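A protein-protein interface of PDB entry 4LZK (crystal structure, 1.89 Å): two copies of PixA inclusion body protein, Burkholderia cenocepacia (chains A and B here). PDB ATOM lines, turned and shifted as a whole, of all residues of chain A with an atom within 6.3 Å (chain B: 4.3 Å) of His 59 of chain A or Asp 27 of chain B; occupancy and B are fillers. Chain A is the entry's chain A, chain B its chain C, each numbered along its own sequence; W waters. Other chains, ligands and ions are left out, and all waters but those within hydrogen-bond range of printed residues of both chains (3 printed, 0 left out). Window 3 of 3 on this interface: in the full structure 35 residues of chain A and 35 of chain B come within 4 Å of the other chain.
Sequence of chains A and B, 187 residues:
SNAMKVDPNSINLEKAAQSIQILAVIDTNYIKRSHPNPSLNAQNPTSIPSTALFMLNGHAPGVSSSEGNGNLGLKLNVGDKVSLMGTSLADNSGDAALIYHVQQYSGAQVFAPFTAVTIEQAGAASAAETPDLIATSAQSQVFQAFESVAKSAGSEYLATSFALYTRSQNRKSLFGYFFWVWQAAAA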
ATOM      1  N   GLN A  18     -23.767  -8.914  35.917  1.00  0.00           N
ATOM      2  CA  GLN A  18     -23.069 -10.119  35.554  1.00  0.00           C
ATOM      3  C   GLN A  18     -21.954 -10.404  36.548  1.00  0.00           C
ATOM      4  O   GLN A  18     -21.506  -9.516  37.330  1.00  0.00           O
ATOM      5  CB  GLN A  18     -22.504  -9.982  34.165  1.00  0.00           C
ATOM      6  CG  GLN A  18     -23.529  -9.603  33.120  1.00  0.00           C
ATOM      7  CD  GLN A  18     -24.560 -10.717  32.874  1.00  0.00           C
ATOM      8  OE1 GLN A  18     -24.248 -11.890  32.990  1.00  0.00           O
ATOM      9  NE2 GLN A  18     -25.731 -10.344  32.446  1.00  0.00           N
ATOM     10  N   ILE A  20     -18.270 -11.961  36.107  1.00  0.00           N
ATOM     11  CA  ILE A  20     -17.361 -12.300  35.047  1.00  0.00           C
ATOM     12  C   ILE A  20     -16.129 -12.967  35.680  1.00  0.00           C
ATOM     13  O   ILE A  20     -15.558 -12.392  36.678  1.00  0.00           O
ATOM     14  CB  ILE A  20     -16.946 -11.025  34.336  1.00  0.00           C
ATOM     15  CG1 ILE A  20     -18.231 -10.354  33.822  1.00  0.00           C
ATOM     16  CG2 ILE A  20     -16.019 -11.330  33.196  1.00  0.00           C
ATOM     17  CD1 ILE A  20     -18.078  -8.888  33.622  1.00  0.00           C
ATOM     18  N   GLN A  21     -15.734 -14.122  35.168  1.00  0.00           N
ATOM     19  CA  GLN A  21     -14.479 -14.757  35.636  1.00  0.00           C
ATOM     20  C   GLN A  21     -13.323 -14.347  34.670  1.00  0.00           C
ATOM     21  O   GLN A  21     -13.504 -14.408  33.412  1.00  0.00           O
ATOM     22  CB  GLN A  21     -14.685 -16.254  35.655  1.00  0.00           C
ATOM     23  CG  GLN A  21     -15.843 -16.772  36.526  1.00  0.00           C
ATOM     24  CD  GLN A  21     -16.019 -18.321  36.385  1.00  0.00           C
ATOM     25  OE1 GLN A  21     -16.218 -18.859  35.287  1.00  0.00           O
ATOM     26  NE2 GLN A  21     -15.962 -18.990  37.447  1.00  0.00           N
ATOM     27  N   ASN A  57     -11.588 -13.955  29.578  1.00  0.00           N
ATOM     28  CA  ASN A  57     -12.777 -13.853  30.439  1.00  0.00           C
ATOM     29  C   ASN A  57     -13.954 -14.584  29.844  1.00  0.00           C
ATOM     30  O   ASN A  57     -14.046 -14.780  28.595  1.00  0.00           O
ATOM     31  CB  ASN A  57     -13.203 -12.393  30.670  1.00  0.00           C
ATOM     32  CG  ASN A  57     -13.592 -11.692  29.414  1.00  0.00           C
ATOM     33  OD1 ASN A  57     -12.679 -11.207  28.714  1.00  0.00           O
ATOM     34  ND2 ASN A  57     -14.886 -11.600  29.117  1.00  0.00           N
ATOM     35  N   GLY A  58     -14.859 -15.018  30.705  1.00  0.00           N
ATOM     36  CA  GLY A  58     -16.093 -15.606  30.189  1.00  0.00           C
ATOM     37  C   GLY A  58     -17.015 -14.600  29.563  1.00  0.00           C
ATOM     38  O   GLY A  58     -17.040 -13.419  29.934  1.00  0.00           O
ATOM     39  N   HIS A  59     -17.718 -15.035  28.529  1.00  0.00           N
ATOM     40  CA  HIS A  59     -18.641 -14.172  27.820  1.00  0.00           C
ATOM     41  C   HIS A  59     -19.906 -13.885  28.669  1.00  0.00           C
ATOM     42  O   HIS A  59     -20.272 -14.656  29.537  1.00  0.00           O
ATOM     43  CB  HIS A  59     -19.029 -14.812  26.484  1.00  0.00           C
ATOM     44  CG  HIS A  59     -17.886 -14.972  25.531  1.00  0.00           C
ATOM     45  ND1 HIS A  59     -17.223 -13.903  24.962  1.00  0.00           N
ATOM     46  CD2 HIS A  59     -17.297 -16.086  25.037  1.00  0.00           C
ATOM     47  CE1 HIS A  59     -16.272 -14.356  24.158  1.00  0.00           C
ATOM     48  NE2 HIS A  59     -16.300 -15.675  24.185  1.00  0.00           N
ATOM     49  N   ALA A  60     -20.544 -12.753  28.395  1.00  0.00           N
ATOM     50  CA  ALA A  60     -21.772 -12.340  29.066  1.00  0.00           C
ATOM     51  C   ALA A  60     -22.380 -11.173  28.290  1.00  0.00           C
ATOM     52  O   ALA A  60     -21.674 -10.454  27.579  1.00  0.00           O
ATOM     53  CB  ALA A  60     -21.451 -11.908  30.501  1.00  0.00           C
ATOM     54  N   PRO A  61     -23.710 -10.940  28.462  1.00  0.00           N
ATOM     55  CA  PRO A  61     -24.384  -9.873  27.757  1.00  0.00           C
ATOM     56  C   PRO A  61     -23.753  -8.484  27.990  1.00  0.00           C
ATOM     57  O   PRO A  61     -23.675  -7.957  29.137  1.00  0.00           O
ATOM     58  CB  PRO A  61     -25.821  -9.977  28.285  1.00  0.00           C
ATOM     59  CG  PRO A  61     -25.982 -11.376  28.677  1.00  0.00           C
ATOM     60  CD  PRO A  61     -24.643 -11.775  29.239  1.00  0.00           C
ATOM     61  N   VAL A  63     -20.653  -7.715  27.677  1.00  0.00           N
ATOM     62  CA  VAL A  63     -19.234  -7.736  28.084  1.00  0.00           C
ATOM     63  C   VAL A  63     -18.420  -8.120  26.840  1.00  0.00           C
ATOM     64  O   VAL A  63     -18.827  -9.026  26.088  1.00  0.00           O
ATOM     65  CB  VAL A  63     -19.020  -8.776  29.198  1.00  0.00           C
ATOM     66  CG1 VAL A  63     -17.536  -8.916  29.518  1.00  0.00           C
ATOM     67  CG2 VAL A  63     -19.892  -8.378  30.377  1.00  0.00           C
ATOM     68  N   SER A  64     -17.324  -7.397  26.599  1.00  0.00           N
ATOM     69  CA  SER A  64     -16.443  -7.792  25.500  1.00  0.00           C
ATOM     70  C   SER A  64     -14.997  -7.613  25.921  1.00  0.00           C
ATOM     71  O   SER A  64     -14.708  -6.998  26.920  1.00  0.00           O
ATOM     72  CB  SER A  64     -16.702  -6.951  24.265  1.00  0.00           C
ATOM     73  OG  SER A  64     -16.223  -5.652  24.470  1.00  0.00           O
ATOM     74  N   SER A  65     -14.085  -8.184  25.155  1.00  0.00           N
ATOM     75  CA  SER A  65     -12.676  -8.037  25.453  1.00  0.00           C
ATOM     76  C   SER A  65     -11.887  -8.423  24.242  1.00  0.00           C
ATOM     77  O   SER A  65     -12.466  -8.973  23.283  1.00  0.00           O
ATOM     78  CB  SER A  65     -12.261  -8.901  26.644  1.00  0.00           C
ATOM     79  OG  SER A  65     -12.358 -10.271  26.266  1.00  0.00           O
ATOM     80  N   GLU A  67      -9.748 -11.164  23.494  1.00  0.00           N
ATOM     81  CA  GLU A  67      -9.529 -12.403  24.282  1.00  0.00           C
ATOM     82  C   GLU A  67      -8.117 -12.889  23.964  1.00  0.00           C
ATOM     83  O   GLU A  67      -7.730 -12.957  22.786  1.00  0.00           O
ATOM     84  CB  GLU A  67     -10.535 -13.507  23.977  1.00  0.00           C
ATOM     85  CG  GLU A  67     -11.978 -13.260  24.411  1.00  0.00           C
ATOM     86  CD  GLU A  67     -12.325 -13.555  25.886  1.00  0.00           C
ATOM     87  OE1 GLU A  67     -11.423 -13.918  26.711  1.00  0.00           O
ATOM     88  OE2 GLU A  67     -13.559 -13.431  26.195  1.00  0.00           O
ATOM     89  N   VAL B  25      -8.211 -23.353  28.226  1.00  0.00           N
ATOM     90  CA  VAL B  25      -9.021 -22.724  29.265  1.00  0.00           C
ATOM     91  C   VAL B  25     -10.485 -22.755  28.858  1.00  0.00           C
ATOM     92  O   VAL B  25     -10.863 -22.095  27.911  1.00  0.00           O
ATOM     93  CB  VAL B  25      -8.549 -21.297  29.544  1.00  0.00           C
ATOM     94  CG1 VAL B  25      -9.451 -20.591  30.601  1.00  0.00           C
ATOM     95  CG2 VAL B  25      -7.076 -21.323  29.961  1.00  0.00           C
ATOM     96  N   ILE B  26     -11.317 -23.465  29.591  1.00  0.00           N
ATOM     97  CA  ILE B  26     -12.645 -23.806  29.135  1.00  0.00           C
ATOM     98  C   ILE B  26     -13.656 -23.015  29.937  1.00  0.00           C
ATOM     99  O   ILE B  26     -13.512 -22.912  31.183  1.00  0.00           O
ATOM    100  CB  ILE B  26     -12.895 -25.321  29.345  1.00  0.00           C
ATOM    101  CG1 ILE B  26     -11.936 -26.080  28.432  1.00  0.00           C
ATOM    102  CG2 ILE B  26     -14.369 -25.711  29.077  1.00  0.00           C
ATOM    103  CD1 ILE B  26     -11.352 -27.293  28.979  1.00  0.00           C
ATOM    104  N   ASP B  27     -14.597 -22.379  29.249  1.00  0.00           N
ATOM    105  CA  ASP B  27     -15.706 -21.607  29.881  1.00  0.00           C
ATOM    106  C   ASP B  27     -16.820 -22.621  30.313  1.00  0.00           C
ATOM    107  O   ASP B  27     -17.762 -22.934  29.573  1.00  0.00           O
ATOM    108  CB  ASP B  27     -16.223 -20.537  28.954  1.00  0.00           C
ATOM    109  CG  ASP B  27     -17.280 -19.574  29.611  1.00  0.00           C
ATOM    110  OD1 ASP B  27     -17.794 -19.856  30.694  1.00  0.00           O
ATOM    111  OD2 ASP B  27     -17.572 -18.535  28.996  1.00  0.00           O
ATOM    112  N   THR B  28     -16.640 -23.178  31.490  1.00  0.00           N
ATOM    113  CA  THR B  28     -17.482 -24.235  31.962  1.00  0.00           C
ATOM    114  C   THR B  28     -18.904 -23.738  32.181  1.00  0.00           C
ATOM    115  O   THR B  28     -19.841 -24.465  31.973  1.00  0.00           O
ATOM    116  CB  THR B  28     -16.896 -24.954  33.209  1.00  0.00           C
ATOM    117  OG1 THR B  28     -16.613 -24.008  34.254  1.00  0.00           O
ATOM    118  CG2 THR B  28     -15.680 -25.734  32.813  1.00  0.00           C
ATOM    119  N   ASN B  29     -19.078 -22.480  32.612  1.00  0.00           N
ATOM    120  CA  ASN B  29     -20.427 -21.901  32.741  1.00  0.00           C
ATOM    121  C   ASN B  29     -21.171 -21.839  31.417  1.00  0.00           C
ATOM    122  O   ASN B  29     -22.366 -22.100  31.339  1.00  0.00           O
ATOM    123  CB  ASN B  29     -20.369 -20.549  33.402  1.00  0.00           C
ATOM    124  CG  ASN B  29     -20.052 -20.666  34.904  1.00  0.00           C
ATOM    125  OD1 ASN B  29     -20.285 -21.708  35.508  1.00  0.00           O
ATOM    126  ND2 ASN B  29     -19.498 -19.609  35.488  1.00  0.00           N
ATOM    127  N   TYR B  30     -20.473 -21.493  30.367  1.00  0.00           N
ATOM    128  CA  TYR B  30     -21.053 -21.477  29.067  1.00  0.00           C
ATOM    129  C   TYR B  30     -21.488 -22.880  28.621  1.00  0.00           C
ATOM    130  O   TYR B  30     -22.622 -23.073  28.075  1.00  0.00           O
ATOM    131  CB  TYR B  30     -20.077 -20.885  28.062  1.00  0.00           C
ATOM    132  CG  TYR B  30     -20.687 -20.914  26.697  1.00  0.00           C
ATOM    133  CD1 TYR B  30     -21.989 -20.455  26.519  1.00  0.00           C
ATOM    134  CD2 TYR B  30     -20.026 -21.468  25.601  1.00  0.00           C
ATOM    135  CE1 TYR B  30     -22.600 -20.517  25.294  1.00  0.00           C
ATOM    136  CE2 TYR B  30     -20.631 -21.519  24.369  1.00  0.00           C
ATOM    137  CZ  TYR B  30     -21.921 -21.033  24.219  1.00  0.00           C
ATOM    138  OH  TYR B  30     -22.573 -21.059  23.003  1.00  0.00           O
ATOM    139  N   ILE B  31     -20.627 -23.878  28.853  1.00  0.00           N
ATOM    140  CA  ILE B  31     -20.950 -25.249  28.507  1.00  0.00           C
ATOM    141  C   ILE B  31     -22.206 -25.736  29.226  1.00  0.00           C
ATOM    142  O   ILE B  31     -23.097 -26.359  28.654  1.00  0.00           O
ATOM    143  CB  ILE B  31     -19.812 -26.234  28.951  1.00  0.00           C
ATOM    144  CG1 ILE B  31     -18.465 -25.861  28.338  1.00  0.00           C
ATOM    145  CG2 ILE B  31     -20.124 -27.638  28.550  1.00  0.00           C
ATOM    146  CD1 ILE B  31     -18.576 -25.505  26.958  1.00  0.00           C
ATOM    147  N   ALA B  52     -16.384 -22.119  22.862  1.00  0.00           N
ATOM    148  CA  ALA B  52     -16.565 -22.324  24.294  1.00  0.00           C
ATOM    149  C   ALA B  52     -15.261 -22.360  25.078  1.00  0.00           C
ATOM    150  O   ALA B  52     -15.267 -22.606  26.271  1.00  0.00           O
ATOM    151  CB  ALA B  52     -17.261 -23.649  24.487  1.00  0.00           C
ATOM    152  N   PHE B  54     -10.712 -21.282  25.132  1.00  0.00           N
ATOM    153  CA  PHE B  54      -9.598 -20.483  24.626  1.00  0.00           C
ATOM    154  C   PHE B  54      -8.334 -21.384  24.702  1.00  0.00           C
ATOM    155  O   PHE B  54      -8.206 -22.185  25.630  1.00  0.00           O
ATOM    156  CB  PHE B  54      -9.419 -19.303  25.528  1.00  0.00           C
ATOM    157  CG  PHE B  54     -10.662 -18.507  25.757  1.00  0.00           C
ATOM    158  CD1 PHE B  54     -11.087 -17.584  24.822  1.00  0.00           C
ATOM    159  CD2 PHE B  54     -11.404 -18.651  26.909  1.00  0.00           C
ATOM    160  CE1 PHE B  54     -12.235 -16.809  25.032  1.00  0.00           C
ATOM    161  CE2 PHE B  54     -12.567 -17.870  27.131  1.00  0.00           C
ATOM    162  CZ  PHE B  54     -12.964 -16.950  26.189  1.00  0.00           C
ATOM    163  N   LEU B  89     -11.982 -21.368  33.716  1.00  0.00           N
ATOM    164  CA  LEU B  89     -11.766 -19.948  33.886  1.00  0.00           C
ATOM    165  C   LEU B  89     -11.491 -19.592  35.344  1.00  0.00           C
ATOM    166  O   LEU B  89     -10.874 -18.552  35.618  1.00  0.00           O
ATOM    167  CB  LEU B  89     -12.927 -19.110  33.336  1.00  0.00           C
ATOM    168  CG  LEU B  89     -12.926 -18.930  31.804  1.00  0.00           C
ATOM    169  CD1 LEU B  89     -14.311 -18.516  31.289  1.00  0.00           C
ATOM    170  CD2 LEU B  89     -11.824 -17.866  31.479  1.00  0.00           C
HETATM  171  O   HOH W   1     -19.625 -17.330  30.587  1.00  0.00           O
HETATM  172  O   HOH W   2     -15.092 -21.755  33.914  1.00  0.00           O
HETATM  173  O   HOH W   3     -17.643 -17.882  33.198  1.00  0.00           O
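Water W3 lies within hydrogen-bond range of OE1 of Gln 21 of chain A (2.7 Å), OD1 of Asp 27 of chain B (3.2 Å) and ND2 of Asn 29 of chain B (3.4 Å). Water W2 lies within hydrogen-bond range of OG1 of Thr 28 of chain B, N of Leu 89 of chain B, O of Ile 26 of chain B and OE1 of Gln 21 of chain A. Water W1 bridges the side-chain carboxylate of Asp 27 of chain B (2.9 Å) and the backbone carbonyl oxygen of His 59 of chain A (2.9 Å).
OD1 of Asn 57 of chain A sits at hydrogen-bond distance from OG of Ser 65 of chain A. N of Asn 57 of chain A sits at hydrogen-bond distance from OE1 of Glu 67 of chain A (2.9 Å). OG of Ser 65 of chain A sits close to OE2 of Glu 67 of chain A (3.4 Å). O of Ile 26 of chain B is in hydrogen-bond range of N of Leu 89 of chain B, at 3.3 Å. OD1 of Asp 27 of chain B sits at hydrogen-bond distance from N of Tyr 30 of chain B, at 3.2 Å. O of Ala 52 of chain B is in hydrogen-bond range of N of Asp 27 of chain B (3.1 Å).
Printed residues of chain A that touch a printed residue of chain B: Gln 21, Asn 57, Gly 58, His 59 and Glu 67. Among the printed residues, no Asp or Glu carboxylate lies within 4 Å of a Lys or Arg side-chain nitrogen of the other chain.
Leu 89 of chain B touches Gln 21 of chain A (CB to OE1, 3.8 Å). Asn 57 of chain A touches Phe 54 of chain B. Asp 27 of chain B touches Gly 58 of chain A (OD2 to CA, 3.5 Å). CA of Gly 58 of chain A touches CD1 of Leu 89 of chain B, 3.6 Å away. His 59 of chain A touches Asp 27 of chain B. Phe 54 of chain B touches Glu 67 of chain A.
No position is printed for both chains. Of the 7 pairs that touch across the chains among the printed residues, none has its exchanged pair printed and touching as well.
Asp 27 of chain B touches just these residues of chain A: Gly 58 and His 59. Printed residues of chain B within 4 Å of Glu 67 of chain A: Phe 54. Of the printed residues of chain A, Asn 29 of chain B touches Gln 21 (3.4 Å). Thr 28 of chain B touches none of the printed residues of chain A. Ala 52 of chain B touches none of the printed residues of chain A. The nearest residue of chain A that does not touch Asp 27 of chain B is Gln 21 of chain A (5.0 Å).
The side-chain amide nitrogen (ND2) of Asn 29 of chain B lies within hydrogen-bond range of the side-chain amide oxygen (OE1) of Gln 21 of chain A, 3.4 Å away.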
